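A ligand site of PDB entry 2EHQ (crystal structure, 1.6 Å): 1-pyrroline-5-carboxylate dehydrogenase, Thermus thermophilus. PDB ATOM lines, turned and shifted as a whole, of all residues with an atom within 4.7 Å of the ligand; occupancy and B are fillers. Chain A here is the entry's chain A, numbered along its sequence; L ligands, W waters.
OG of Ser 261 lies within hydrogen-bond range of N of Val 264 (3.2 Å).
O of Ser 491 is in hydrogen-bond range of N of Thr 289 (2.9 Å).
O of Gly 240 is in hydrogen-bond range of N of Ala 245 (2.9 Å).
The backbone carbonyl oxygen of Lys 207 lies within hydrogen-bond range of the backbone NH of Ala 181, at 3.1 Å.
The backbone carbonyl oxygen (O) of Ala 181 sits close to the backbone NH (N) of Ala 209 (3.4 Å).
NZ of Lys 207 sits at hydrogen-bond distance from O of Gly 238, 3.0 Å away.
N of Gly 260 lies within hydrogen-bond range of O of Glu 288 (3.0 Å).
O of Ile 180 lies within hydrogen-bond range of N of Thr 259.
An oxygen (O15) of the ligand sits at hydrogen-bond distance from the backbone NH (N) of Glu 210 (2.9 Å).
OE2 of Glu 210 sits close to O16 of the ligand (2.5 Å).
An oxygen (O12) of the ligand sits at hydrogen-bond distance from the side-chain carboxylate of Glu 417 (2.6 Å).
N of Ser 261 is in hydrogen-bond range of O2 of the ligand (2.8 Å).
The side-chain hydroxyl of Ser 261 lies within hydrogen-bond range of an oxygen (O2) of the ligand, at 2.6 Å.
O of Thr 289 lies within hydrogen-bond range of N7 of the ligand (2.7 Å).
N of Gly 240 lies within hydrogen-bond range of O16 of the ligand (2.7 Å).
An oxygen (O5) of the ligand sits at hydrogen-bond distance from the backbone carbonyl oxygen (O) of Ala 181.
The indole nitrogen (NE1) of Trp 183 lies within hydrogen-bond range of an oxygen (O9) of the ligand, at 2.8 Å.
An oxygen (O16) of the ligand is in salt-bridge range of the side-chain amino group (NZ) of Lys 207 (3.1 Å).
SG of Cys 322 lies close to O14 of the ligand, 3.7 Å away.
The backbone carbonyl oxygen of Gly 238 lies close to an oxygen (O16) of the ligand, at 3.5 Å.
An oxygen (O11) of the ligand sits close to the backbone carbonyl oxygen of Gly 260 (3.2 Å).
Merely in contact with the ligand: Thr 259 (3.0 Å), Ile 180 (3.2 Å), Asn 184 (3.2 Å), Phe 419 (3.2 Å), Gly 290 (3.2 Å), Phe 485 (3.3 Å), Glu 288 (3.3 Å), Phe 258 (3.4 Å), Val 264 (3.4 Å), Ile 189 (3.4 Å), Glu 241 (3.4 Å), Pro 182 (3.4 Å), Ala 209 (3.5 Å), Ala 245 (3.6 Å), Val 239 (3.6 Å), Gly 244 (3.7 Å), Leu 445 (3.7 Å), Ile 268 (3.9 Å) and Pro 208 (3.98 Å).
Along chain A the residues within 4 Å of the ligand span positions 180 to 485.
Water W7 lies within hydrogen-bond range of N of Glu 241 (2.9 Å), O17 of the ligand (2.9 Å) and N of Gly 240 (3.4 Å).
Water W4 lies within hydrogen-bond range of the side-chain carboxylate of Glu 241 (2.5 Å), a nitrogen (N3) of the ligand (2.9 Å) and the side-chain amino group of Lys 267 (3.4 Å).
Water W9 bridges the side-chain sulfur (SG) of Cys 322 (2.7 Å) and the side-chain amide nitrogen (ND2) of Asn 184 (2.8 Å).
Water W2 lies within hydrogen-bond range of OE1 of Glu 288 (2.6 Å), O of Ser 491 (2.8 Å) and N7 of the ligand (3.1 Å).
Water W3 lies within hydrogen-bond range of the backbone NH (N) of Glu 210 (3.3 Å) and an oxygen (O15) of the ligand (3.4 Å).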
ATOM      1  N   ILE A 180     -15.686  -5.053  16.666  1.00  0.00           N
ATOM      2  CA  ILE A 180     -15.577  -4.439  15.329  1.00  0.00           C
ATOM      3  C   ILE A 180     -15.866  -5.547  14.321  1.00  0.00           C
ATOM      4  O   ILE A 180     -15.167  -6.570  14.307  1.00  0.00           O
ATOM      5  CB  ILE A 180     -14.202  -3.809  15.130  1.00  0.00           C
ATOM      6  CG1 ILE A 180     -13.987  -2.686  16.169  1.00  0.00           C
ATOM      7  CG2 ILE A 180     -14.064  -3.264  13.718  1.00  0.00           C
ATOM      8  CD1 ILE A 180     -12.625  -2.036  16.123  1.00  0.00           C
ATOM      9  N   ALA A 181     -16.924  -5.368  13.533  1.00  0.00           N
ATOM     10  CA  ALA A 181     -17.543  -6.469  12.797  1.00  0.00           C
ATOM     11  C   ALA A 181     -17.483  -6.309  11.278  1.00  0.00           C
ATOM     12  O   ALA A 181     -17.358  -5.177  10.758  1.00  0.00           O
ATOM     13  CB  ALA A 181     -18.988  -6.632  13.266  1.00  0.00           C
ATOM     14  N   PRO A 182     -17.571  -7.424  10.549  1.00  0.00           N
ATOM     15  CA  PRO A 182     -17.567  -7.413   9.094  1.00  0.00           C
ATOM     16  C   PRO A 182     -18.952  -7.321   8.469  1.00  0.00           C
ATOM     17  O   PRO A 182     -19.964  -7.543   9.156  1.00  0.00           O
ATOM     18  CB  PRO A 182     -16.967  -8.778   8.750  1.00  0.00           C
ATOM     19  CG  PRO A 182     -17.516  -9.675   9.809  1.00  0.00           C
ATOM     20  CD  PRO A 182     -17.600  -8.808  11.075  1.00  0.00           C
ATOM     21  N   TRP A 183     -19.002  -6.991   7.169  1.00  0.00           N
ATOM     22  CA  TRP A 183     -20.271  -6.908   6.432  1.00  0.00           C
ATOM     23  C   TRP A 183     -20.797  -8.242   5.929  1.00  0.00           C
ATOM     24  O   TRP A 183     -21.967  -8.328   5.536  1.00  0.00           O
ATOM     25  CB  TRP A 183     -20.192  -5.926   5.262  1.00  0.00           C
ATOM     26  CG  TRP A 183     -19.030  -6.194   4.351  1.00  0.00           C
ATOM     27  CD1 TRP A 183     -17.832  -5.560   4.377  1.00  0.00           C
ATOM     28  CD2 TRP A 183     -18.948  -7.169   3.296  1.00  0.00           C
ATOM     29  NE1 TRP A 183     -16.995  -6.065   3.403  1.00  0.00           N
ATOM     30  CE2 TRP A 183     -17.657  -7.050   2.721  1.00  0.00           C
ATOM     31  CE3 TRP A 183     -19.840  -8.127   2.766  1.00  0.00           C
ATOM     32  CZ2 TRP A 183     -17.236  -7.838   1.655  1.00  0.00           C
ATOM     33  CZ3 TRP A 183     -19.414  -8.920   1.694  1.00  0.00           C
ATOM     34  CH2 TRP A 183     -18.114  -8.774   1.169  1.00  0.00           C
ATOM     35  N   ASN A 184     -19.962  -9.275   5.923  1.00  0.00           N
ATOM     36  CA  ASN A 184     -20.367 -10.513   5.218  1.00  0.00           C
ATOM     37  C   ASN A 184     -21.264 -11.459   6.021  1.00  0.00           C
ATOM     38  O   ASN A 184     -22.018 -12.230   5.422  1.00  0.00           O
ATOM     39  CB  ASN A 184     -19.163 -11.250   4.604  1.00  0.00           C
ATOM     40  CG  ASN A 184     -18.327 -11.944   5.643  1.00  0.00           C
ATOM     41  OD1 ASN A 184     -18.159 -11.444   6.770  1.00  0.00           O
ATOM     42  ND2 ASN A 184     -17.788 -13.115   5.282  1.00  0.00           N
ATOM     43  N   ILE A 189     -22.159 -12.870  12.911  1.00  0.00           N
ATOM     44  CA  ILE A 189     -20.874 -12.581  13.577  1.00  0.00           C
ATOM     45  C   ILE A 189     -20.961 -11.343  14.472  1.00  0.00           C
ATOM     46  O   ILE A 189     -20.374 -11.300  15.552  1.00  0.00           O
ATOM     47  CB  ILE A 189     -19.756 -12.481  12.541  1.00  0.00           C
ATOM     48  CG1 ILE A 189     -19.446 -13.904  12.023  1.00  0.00           C
ATOM     49  CG2 ILE A 189     -18.500 -11.878  13.143  1.00  0.00           C
ATOM     50  CD1 ILE A 189     -18.444 -13.961  10.886  1.00  0.00           C
ATOM     51  N   LYS A 207     -19.203  -1.780  16.736  1.00  0.00           N
ATOM     52  CA  LYS A 207     -19.025  -0.988  15.519  1.00  0.00           C
ATOM     53  C   LYS A 207     -19.333  -1.872  14.291  1.00  0.00           C
ATOM     54  O   LYS A 207     -18.479  -2.655  13.880  1.00  0.00           O
ATOM     55  CB  LYS A 207     -17.561  -0.502  15.469  1.00  0.00           C
ATOM     56  CG  LYS A 207     -17.318   0.877  14.823  1.00  0.00           C
ATOM     57  CD  LYS A 207     -17.742   0.915  13.348  1.00  0.00           C
ATOM     58  CE  LYS A 207     -16.790   0.130  12.456  1.00  0.00           C
ATOM     59  NZ  LYS A 207     -17.230   0.253  11.021  1.00  0.00           N
ATOM     60  N   PRO A 208     -20.545  -1.758  13.711  1.00  0.00           N
ATOM     61  CA  PRO A 208     -20.863  -2.572  12.527  1.00  0.00           C
ATOM     62  C   PRO A 208     -20.114  -2.085  11.303  1.00  0.00           C
ATOM     63  O   PRO A 208     -19.722  -0.904  11.240  1.00  0.00           O
ATOM     64  CB  PRO A 208     -22.349  -2.320  12.320  1.00  0.00           C
ATOM     65  CG  PRO A 208     -22.533  -0.896  12.857  1.00  0.00           C
ATOM     66  CD  PRO A 208     -21.645  -0.842  14.066  1.00  0.00           C
ATOM     67  N   ALA A 209     -19.914  -2.980  10.338  1.00  0.00           N
ATOM     68  CA  ALA A 209     -19.322  -2.613   9.056  1.00  0.00           C
ATOM     69  C   ALA A 209     -20.226  -1.614   8.336  1.00  0.00           C
ATOM     70  O   ALA A 209     -21.449  -1.649   8.456  1.00  0.00           O
ATOM     71  CB  ALA A 209     -19.111  -3.849   8.210  1.00  0.00           C
ATOM     72  N   GLU A 210     -19.615  -0.709   7.592  1.00  0.00           N
ATOM     73  CA  GLU A 210     -20.370   0.342   6.902  1.00  0.00           C
ATOM     74  C   GLU A 210     -21.478  -0.148   5.992  1.00  0.00           C
ATOM     75  O   GLU A 210     -22.544   0.482   5.910  1.00  0.00           O
ATOM     76  CB  GLU A 210     -19.411   1.239   6.118  1.00  0.00           C
ATOM     77  CG  GLU A 210     -18.639   2.168   7.021  1.00  0.00           C
ATOM     78  CD  GLU A 210     -17.707   3.083   6.278  1.00  0.00           C
ATOM     79  OE1 GLU A 210     -18.162   3.798   5.350  1.00  0.00           O
ATOM     80  OE2 GLU A 210     -16.517   3.106   6.631  1.00  0.00           O
ATOM     81  N   GLY A 238     -20.231   3.753  12.119  1.00  0.00           N
ATOM     82  CA  GLY A 238     -19.239   4.774  11.815  1.00  0.00           C
ATOM     83  C   GLY A 238     -18.105   4.182  11.021  1.00  0.00           C
ATOM     84  O   GLY A 238     -18.159   3.033  10.587  1.00  0.00           O
ATOM     85  N   VAL A 239     -17.077   5.005  10.813  1.00  0.00           N
ATOM     86  CA  VAL A 239     -15.963   4.650   9.952  1.00  0.00           C
ATOM     87  C   VAL A 239     -14.909   3.908  10.765  1.00  0.00           C
ATOM     88  O   VAL A 239     -14.348   4.448  11.703  1.00  0.00           O
ATOM     89  CB  VAL A 239     -15.368   5.907   9.289  1.00  0.00           C
ATOM     90  CG1 VAL A 239     -14.171   5.532   8.459  1.00  0.00           C
ATOM     91  CG2 VAL A 239     -16.412   6.573   8.389  1.00  0.00           C
ATOM     92  N   GLY A 240     -14.649   2.653  10.396  1.00  0.00           N
ATOM     93  CA  GLY A 240     -13.679   1.834  11.115  1.00  0.00           C
ATOM     94  C   GLY A 240     -12.319   2.477  11.319  1.00  0.00           C
ATOM     95  O   GLY A 240     -11.806   2.490  12.438  1.00  0.00           O
ATOM     96  N   GLU A 241     -11.748   3.032  10.243  1.00  0.00           N
ATOM     97  CA  GLU A 241     -10.428   3.667  10.318  1.00  0.00           C
ATOM     98  C   GLU A 241     -10.395   4.933  11.171  1.00  0.00           C
ATOM     99  O   GLU A 241      -9.313   5.436  11.500  1.00  0.00           O
ATOM    100  CB  GLU A 241      -9.847   3.956   8.914  1.00  0.00           C
ATOM    101  CG  GLU A 241      -9.321   2.737   8.171  1.00  0.00           C
ATOM    102  CD  GLU A 241      -8.695   3.098   6.829  1.00  0.00           C
ATOM    103  OE1 GLU A 241      -9.294   3.909   6.074  1.00  0.00           O
ATOM    104  OE2 GLU A 241      -7.608   2.565   6.513  1.00  0.00           O
ATOM    105  N   GLY A 244     -13.379   3.334  14.893  1.00  0.00           N
ATOM    106  CA  GLY A 244     -12.898   1.993  15.272  1.00  0.00           C
ATOM    107  C   GLY A 244     -11.472   2.028  15.790  1.00  0.00           C
ATOM    108  O   GLY A 244     -11.174   1.537  16.892  1.00  0.00           O
ATOM    109  N   ALA A 245     -10.584   2.654  15.016  1.00  0.00           N
ATOM    110  CA  ALA A 245      -9.184   2.813  15.447  1.00  0.00           C
ATOM    111  C   ALA A 245      -9.111   3.605  16.764  1.00  0.00           C
ATOM    112  O   ALA A 245      -8.309   3.279  17.655  1.00  0.00           O
ATOM    113  CB  ALA A 245      -8.349   3.498  14.357  1.00  0.00           C
ATOM    114  N   VAL A 248      -9.888   1.147  19.487  1.00  0.00           N
ATOM    115  CA  VAL A 248      -8.796   0.171  19.575  1.00  0.00           C
ATOM    116  C   VAL A 248      -7.601   0.732  20.355  1.00  0.00           C
ATOM    117  O   VAL A 248      -7.002   0.030  21.176  1.00  0.00           O
ATOM    118  CB  VAL A 248      -8.338  -0.318  18.161  1.00  0.00           C
ATOM    119  CG1 VAL A 248      -7.030  -1.080  18.261  1.00  0.00           C
ATOM    120  CG2 VAL A 248      -9.434  -1.196  17.529  1.00  0.00           C
ATOM    121  N   PHE A 258     -12.489  -8.598  17.145  1.00  0.00           N
ATOM    122  CA  PHE A 258     -12.468  -8.191  15.745  1.00  0.00           C
ATOM    123  C   PHE A 258     -12.597  -9.378  14.812  1.00  0.00           C
ATOM    124  O   PHE A 258     -11.938 -10.395  15.003  1.00  0.00           O
ATOM    125  CB  PHE A 258     -11.184  -7.415  15.428  1.00  0.00           C
ATOM    126  CG  PHE A 258     -10.971  -7.162  13.954  1.00  0.00           C
ATOM    127  CD1 PHE A 258     -11.560  -6.051  13.334  1.00  0.00           C
ATOM    128  CD2 PHE A 258     -10.170  -8.023  13.183  1.00  0.00           C
ATOM    129  CE1 PHE A 258     -11.359  -5.816  11.980  1.00  0.00           C
ATOM    130  CE2 PHE A 258      -9.960  -7.785  11.820  1.00  0.00           C
ATOM    131  CZ  PHE A 258     -10.563  -6.685  11.213  1.00  0.00           C
ATOM    132  N   THR A 259     -13.445  -9.215  13.809  1.00  0.00           N
ATOM    133  CA  THR A 259     -13.488 -10.120  12.673  1.00  0.00           C
ATOM    134  C   THR A 259     -13.481  -9.270  11.404  1.00  0.00           C
ATOM    135  O   THR A 259     -14.285  -8.343  11.272  1.00  0.00           O
ATOM    136  CB  THR A 259     -14.727 -11.030  12.740  1.00  0.00           C
ATOM    137  OG1 THR A 259     -14.706 -11.768  13.967  1.00  0.00           O
ATOM    138  CG2 THR A 259     -14.743 -11.980  11.587  1.00  0.00           C
ATOM    139  N   GLY A 260     -12.590  -9.591  10.482  1.00  0.00           N
ATOM    140  CA  GLY A 260     -12.414  -8.772   9.270  1.00  0.00           C
ATOM    141  C   GLY A 260     -11.155  -9.135   8.521  1.00  0.00           C
ATOM    142  O   GLY A 260     -10.651 -10.255   8.640  1.00  0.00           O
ATOM    143  N   SER A 261     -10.643  -8.200   7.722  1.00  0.00           N
ATOM    144  CA  SER A 261      -9.504  -8.473   6.860  1.00  0.00           C
ATOM    145  C   SER A 261      -8.218  -8.638   7.655  1.00  0.00           C
ATOM    146  O   SER A 261      -8.044  -8.081   8.753  1.00  0.00           O
ATOM    147  CB  SER A 261      -9.301  -7.336   5.851  1.00  0.00           C
ATOM    148  OG  SER A 261      -8.924  -6.145   6.522  1.00  0.00           O
ATOM    149  N   LEU A 262      -7.290  -9.399   7.065  1.00  0.00           N
ATOM    150  CA  LEU A 262      -5.950  -9.532   7.618  1.00  0.00           C
ATOM    151  C   LEU A 262      -5.257  -8.171   7.745  1.00  0.00           C
ATOM    152  O   LEU A 262      -4.635  -7.891   8.776  1.00  0.00           O
ATOM    153  CB  LEU A 262      -5.098 -10.492   6.788  1.00  0.00           C
ATOM    154  CG  LEU A 262      -3.630 -10.596   7.223  1.00  0.00           C
ATOM    155  CD1 LEU A 262      -3.502 -11.145   8.646  1.00  0.00           C
ATOM    156  CD2 LEU A 262      -2.854 -11.448   6.256  1.00  0.00           C
ATOM    157  N   VAL A 264      -6.458  -5.191   8.338  1.00  0.00           N
ATOM    158  CA  VAL A 264      -6.949  -4.450   9.493  1.00  0.00           C
ATOM    159  C   VAL A 264      -6.591  -5.197  10.786  1.00  0.00           C
ATOM    160  O   VAL A 264      -6.150  -4.586  11.776  1.00  0.00           O
ATOM    161  CB  VAL A 264      -8.470  -4.169   9.376  1.00  0.00           C
ATOM    162  CG1 VAL A 264      -8.986  -3.535  10.654  1.00  0.00           C
ATOM    163  CG2 VAL A 264      -8.729  -3.216   8.191  1.00  0.00           C
ATOM    164  N   LYS A 267      -3.128  -4.418  12.011  1.00  0.00           N
ATOM    165  CA  LYS A 267      -3.063  -3.112  12.644  1.00  0.00           C
ATOM    166  C   LYS A 267      -3.642  -3.125  14.049  1.00  0.00           C
ATOM    167  O   LYS A 267      -3.102  -2.488  14.962  1.00  0.00           O
ATOM    168  CB  LYS A 267      -3.782  -2.064  11.809  1.00  0.00           C
ATOM    169  CG  LYS A 267      -3.129  -1.806  10.485  1.00  0.00           C
ATOM    170  CD  LYS A 267      -4.008  -0.927   9.617  1.00  0.00           C
ATOM    171  CE  LYS A 267      -3.276  -0.566   8.326  1.00  0.00           C
ATOM    172  NZ  LYS A 267      -4.126   0.333   7.516  1.00  0.00           N
ATOM    173  N   ILE A 268      -4.757  -3.842  14.227  1.00  0.00           N
ATOM    174  CA  ILE A 268      -5.430  -3.927  15.507  1.00  0.00           C
ATOM    175  C   ILE A 268      -4.582  -4.694  16.526  1.00  0.00           C
ATOM    176  O   ILE A 268      -4.414  -4.271  17.672  1.00  0.00           O
ATOM    177  CB  ILE A 268      -6.820  -4.559  15.346  1.00  0.00           C
ATOM    178  CG1 ILE A 268      -7.738  -3.577  14.596  1.00  0.00           C
ATOM    179  CG2 ILE A 268      -7.425  -4.936  16.708  1.00  0.00           C
ATOM    180  CD1 ILE A 268      -9.121  -4.113  14.356  1.00  0.00           C
ATOM    181  N   GLU A 288      -9.974 -12.379  14.043  1.00  0.00           N
ATOM    182  CA  GLU A 288     -10.243 -13.500  13.180  1.00  0.00           C
ATOM    183  C   GLU A 288     -10.257 -12.912  11.765  1.00  0.00           C
ATOM    184  O   GLU A 288     -11.079 -12.042  11.436  1.00  0.00           O
ATOM    185  CB  GLU A 288     -11.532 -14.163  13.654  1.00  0.00           C
ATOM    186  CG  GLU A 288     -11.418 -14.565  15.161  1.00  0.00           C
ATOM    187  CD  GLU A 288     -10.355 -15.646  15.431  1.00  0.00           C
ATOM    188  OE1 GLU A 288     -10.369 -16.659  14.698  1.00  0.00           O
ATOM    189  OE2 GLU A 288      -9.552 -15.496  16.373  1.00  0.00           O
ATOM    190  N   THR A 289      -9.292 -13.362  10.980  1.00  0.00           N
ATOM    191  CA  THR A 289      -8.952 -12.711   9.746  1.00  0.00           C
ATOM    192  C   THR A 289      -9.323 -13.629   8.588  1.00  0.00           C
ATOM    193  O   THR A 289     -10.120 -14.553   8.760  1.00  0.00           O
ATOM    194  CB  THR A 289      -7.458 -12.295   9.771  1.00  0.00           C
ATOM    195  OG1 THR A 289      -6.661 -13.397  10.236  1.00  0.00           O
ATOM    196  CG2 THR A 289      -7.260 -11.107  10.736  1.00  0.00           C
ATOM    197  N   GLY A 290      -8.772 -13.358   7.403  1.00  0.00           N
ATOM    198  CA  GLY A 290      -9.177 -14.048   6.205  1.00  0.00           C
ATOM    199  C   GLY A 290      -8.645 -15.454   6.031  1.00  0.00           C
ATOM    200  O   GLY A 290      -7.963 -16.007   6.914  1.00  0.00           O
ATOM    201  N   GLY A 291      -8.975 -16.030   4.885  1.00  0.00           N
ATOM    202  CA  GLY A 291      -8.523 -17.361   4.519  1.00  0.00           C
ATOM    203  C   GLY A 291      -8.229 -17.441   3.042  1.00  0.00           C
ATOM    204  O   GLY A 291      -8.742 -16.656   2.245  1.00  0.00           O
ATOM    205  N   CYS A 322     -15.083 -16.001   4.585  1.00  0.00           N
ATOM    206  CA  CYS A 322     -13.736 -16.308   5.071  1.00  0.00           C
ATOM    207  C   CYS A 322     -13.444 -17.797   4.909  1.00  0.00           C
ATOM    208  O   CYS A 322     -12.288 -18.189   4.862  1.00  0.00           O
ATOM    209  CB  CYS A 322     -13.566 -15.918   6.529  1.00  0.00           C
ATOM    210  SG  CYS A 322     -14.727 -16.698   7.642  1.00  0.00           S
ATOM    211  N   GLU A 417      -6.347 -13.280  -0.655  1.00  0.00           N
ATOM    212  CA  GLU A 417      -7.796 -13.445  -0.501  1.00  0.00           C
ATOM    213  C   GLU A 417      -8.549 -12.458  -1.380  1.00  0.00           C
ATOM    214  O   GLU A 417      -8.499 -11.240  -1.143  1.00  0.00           O
ATOM    215  CB  GLU A 417      -8.201 -13.288   0.965  1.00  0.00           C
ATOM    216  CG  GLU A 417      -9.666 -13.580   1.203  1.00  0.00           C
ATOM    217  CD  GLU A 417     -10.089 -13.326   2.614  1.00  0.00           C
ATOM    218  OE1 GLU A 417      -9.762 -12.244   3.154  1.00  0.00           O
ATOM    219  OE2 GLU A 417     -10.764 -14.217   3.185  1.00  0.00           O
ATOM    220  N   PHE A 419     -11.999 -12.745  -2.162  1.00  0.00           N
ATOM    221  CA  PHE A 419     -13.303 -12.482  -1.546  1.00  0.00           C
ATOM    222  C   PHE A 419     -14.391 -12.170  -2.582  1.00  0.00           C
ATOM    223  O   PHE A 419     -15.209 -11.274  -2.386  1.00  0.00           O
ATOM    224  CB  PHE A 419     -13.196 -11.366  -0.488  1.00  0.00           C
ATOM    225  CG  PHE A 419     -13.961 -11.656   0.758  1.00  0.00           C
ATOM    226  CD1 PHE A 419     -13.575 -12.725   1.575  1.00  0.00           C
ATOM    227  CD2 PHE A 419     -15.022 -10.862   1.160  1.00  0.00           C
ATOM    228  CE1 PHE A 419     -14.255 -13.019   2.741  1.00  0.00           C
ATOM    229  CE2 PHE A 419     -15.708 -11.132   2.348  1.00  0.00           C
ATOM    230  CZ  PHE A 419     -15.335 -12.218   3.135  1.00  0.00           C
ATOM    231  N   LEU A 445      -7.477 -21.237   7.680  1.00  0.00           N
ATOM    232  CA  LEU A 445      -8.839 -21.176   8.191  1.00  0.00           C
ATOM    233  C   LEU A 445      -9.660 -22.436   7.934  1.00  0.00           C
ATOM    234  O   LEU A 445      -9.881 -23.224   8.860  1.00  0.00           O
ATOM    235  CB  LEU A 445      -9.578 -19.933   7.673  1.00  0.00           C
ATOM    236  CG  LEU A 445     -10.863 -19.562   8.406  1.00  0.00           C
ATOM    237  CD1 LEU A 445     -10.793 -19.731   9.926  1.00  0.00           C
ATOM    238  CD2 LEU A 445     -11.248 -18.147   8.069  1.00  0.00           C
ATOM    239  N   PHE A 485     -15.329 -22.708  15.453  1.00  0.00           N
ATOM    240  CA  PHE A 485     -14.854 -22.020  14.249  1.00  0.00           C
ATOM    241  C   PHE A 485     -13.735 -21.010  14.486  1.00  0.00           C
ATOM    242  O   PHE A 485     -13.870 -20.092  15.295  1.00  0.00           O
ATOM    243  CB  PHE A 485     -16.004 -21.349  13.491  1.00  0.00           C
ATOM    244  CG  PHE A 485     -15.587 -20.801  12.159  1.00  0.00           C
ATOM    245  CD1 PHE A 485     -15.380 -21.667  11.093  1.00  0.00           C
ATOM    246  CD2 PHE A 485     -15.362 -19.437  11.970  1.00  0.00           C
ATOM    247  CE1 PHE A 485     -14.971 -21.202   9.844  1.00  0.00           C
ATOM    248  CE2 PHE A 485     -14.960 -18.939  10.703  1.00  0.00           C
ATOM    249  CZ  PHE A 485     -14.755 -19.823   9.651  1.00  0.00           C
ATOM    250  N   SER A 491      -4.825 -16.495   9.594  1.00  0.00           N
ATOM    251  CA  SER A 491      -6.284 -16.497   9.692  1.00  0.00           C
ATOM    252  C   SER A 491      -6.761 -16.069  11.077  1.00  0.00           C
ATOM    253  O   SER A 491      -7.971 -15.959  11.310  1.00  0.00           O
ATOM    254  CB  SER A 491      -6.869 -17.847   9.312  1.00  0.00           C
ATOM    255  OG  SER A 491      -6.634 -18.110   7.927  1.00  0.00           O
HETATM  256  P1  LIG L   1     -12.458  -5.023   7.011  1.00  0.00           P
HETATM  257  O1  LIG L   1     -12.230  -4.115   5.884  1.00  0.00           O
HETATM  258  O2  LIG L   1     -11.214  -5.475   7.661  1.00  0.00           O
HETATM  259  O3  LIG L   1     -13.462  -4.350   8.037  1.00  0.00           O
HETATM  260  C1  LIG L   1     -13.891  -5.055   9.168  1.00  0.00           C
HETATM  261  C2  LIG L   1     -14.315  -4.023  10.209  1.00  0.00           C
HETATM  262  O4  LIG L   1     -13.194  -3.288  10.663  1.00  0.00           O
HETATM  263  C3  LIG L   1     -15.311  -2.998   9.675  1.00  0.00           C
HETATM  264  O5  LIG L   1     -16.203  -2.688  10.721  1.00  0.00           O
HETATM  265  C4  LIG L   1     -14.418  -1.811   9.358  1.00  0.00           C
HETATM  266  O6  LIG L   1     -15.072  -0.568   9.381  1.00  0.00           O
HETATM  267  C5  LIG L   1     -13.444  -1.884  10.514  1.00  0.00           C
HETATM  268  N1  LIG L   1     -12.172  -1.223  10.223  1.00  0.00           N
HETATM  269  C6  LIG L   1     -11.594  -0.902   9.018  1.00  0.00           C
HETATM  270  N2  LIG L   1     -10.385  -0.333   9.261  1.00  0.00           N
HETATM  271  C7  LIG L   1     -10.198  -0.296  10.608  1.00  0.00           C
HETATM  272  C8  LIG L   1      -9.160   0.147  11.428  1.00  0.00           C
HETATM  273  N3  LIG L   1      -8.022   0.642  10.928  1.00  0.00           N
HETATM  274  N4  LIG L   1      -9.280   0.028  12.787  1.00  0.00           N
HETATM  275  C9  LIG L   1     -10.420  -0.523  13.352  1.00  0.00           C
HETATM  276  N5  LIG L   1     -11.442  -0.977  12.558  1.00  0.00           N
HETATM  277  C10 LIG L   1     -11.312  -0.868  11.216  1.00  0.00           C
HETATM  278  O7  LIG L   1     -13.212  -6.395   6.622  1.00  0.00           O
HETATM  279  P2  LIG L   1     -14.619  -6.520   5.841  1.00  0.00           P
HETATM  280  O8  LIG L   1     -15.715  -5.921   6.615  1.00  0.00           O
HETATM  281  O9  LIG L   1     -14.378  -6.153   4.422  1.00  0.00           O
HETATM  282  O10 LIG L   1     -14.878  -8.104   5.915  1.00  0.00           O
HETATM  283  C11 LIG L   1     -14.278  -8.994   5.013  1.00  0.00           C
HETATM  284  C12 LIG L   1     -13.028  -9.619   5.627  1.00  0.00           C
HETATM  285  O11 LIG L   1     -13.364 -10.194   6.878  1.00  0.00           O
HETATM  286  C13 LIG L   1     -12.479 -10.763   4.773  1.00  0.00           C
HETATM  287  O12 LIG L   1     -11.065 -10.693   4.753  1.00  0.00           O
HETATM  288  C14 LIG L   1     -12.957 -11.994   5.507  1.00  0.00           C
HETATM  289  O13 LIG L   1     -12.149 -13.131   5.322  1.00  0.00           O
HETATM  290  C15 LIG L   1     -12.909 -11.533   6.950  1.00  0.00           C
HETATM  291  N6  LIG L   1     -13.775 -12.360   7.793  1.00  0.00           N
HETATM  292  C16 LIG L   1     -13.191 -13.244   8.649  1.00  0.00           C
HETATM  293  C17 LIG L   1     -13.994 -14.048   9.448  1.00  0.00           C
HETATM  294  C18 LIG L   1     -13.413 -15.070  10.375  1.00  0.00           C
HETATM  295  O14 LIG L   1     -14.272 -15.753  11.227  1.00  0.00           O
HETATM  296  N7  LIG L   1     -12.105 -15.324  10.365  1.00  0.00           N
HETATM  297  C19 LIG L   1     -15.396 -13.937   9.365  1.00  0.00           C
HETATM  298  C20 LIG L   1     -15.969 -13.019   8.489  1.00  0.00           C
HETATM  299  C21 LIG L   1     -15.145 -12.235   7.695  1.00  0.00           C
HETATM  300  P3  LIG L   1     -15.589   0.014   7.971  1.00  0.00           P
HETATM  301  O15 LIG L   1     -16.706  -0.863   7.499  1.00  0.00           O
HETATM  302  O16 LIG L   1     -16.009   1.414   8.371  1.00  0.00           O
HETATM  303  O17 LIG L   1     -14.403   0.013   7.041  1.00  0.00           O
HETATM  304  O   HOH W   1     -12.141  -5.831   3.082  1.00  0.00           O
HETATM  305  O   HOH W   2     -10.349 -17.203  12.159  1.00  0.00           O
HETATM  306  O   HOH W   3     -18.473  -2.217   4.879  1.00  0.00           O
HETATM  307  O   HOH W   4      -7.479   0.550   8.052  1.00  0.00           O
HETATM  308  O   HOH W   5     -14.011  -3.530   4.028  1.00  0.00           O
HETATM  309  O   HOH W   6     -16.074  -3.123   5.933  1.00  0.00           O
HETATM  310  O   HOH W   7     -12.738   2.292   7.645  1.00  0.00           O
HETATM  311  O   HOH W   8     -15.208 -16.119  13.416  1.00  0.00           O
HETATM  312  O   HOH W   9     -16.742 -15.294   6.637  1.00  0.00           O
HETATM  313  O   HOH W  10     -11.080  -8.444   2.717  1.00  0.00           O
HETATM  314  O   HOH W  11     -12.423  -1.398   5.976  1.00  0.00           O
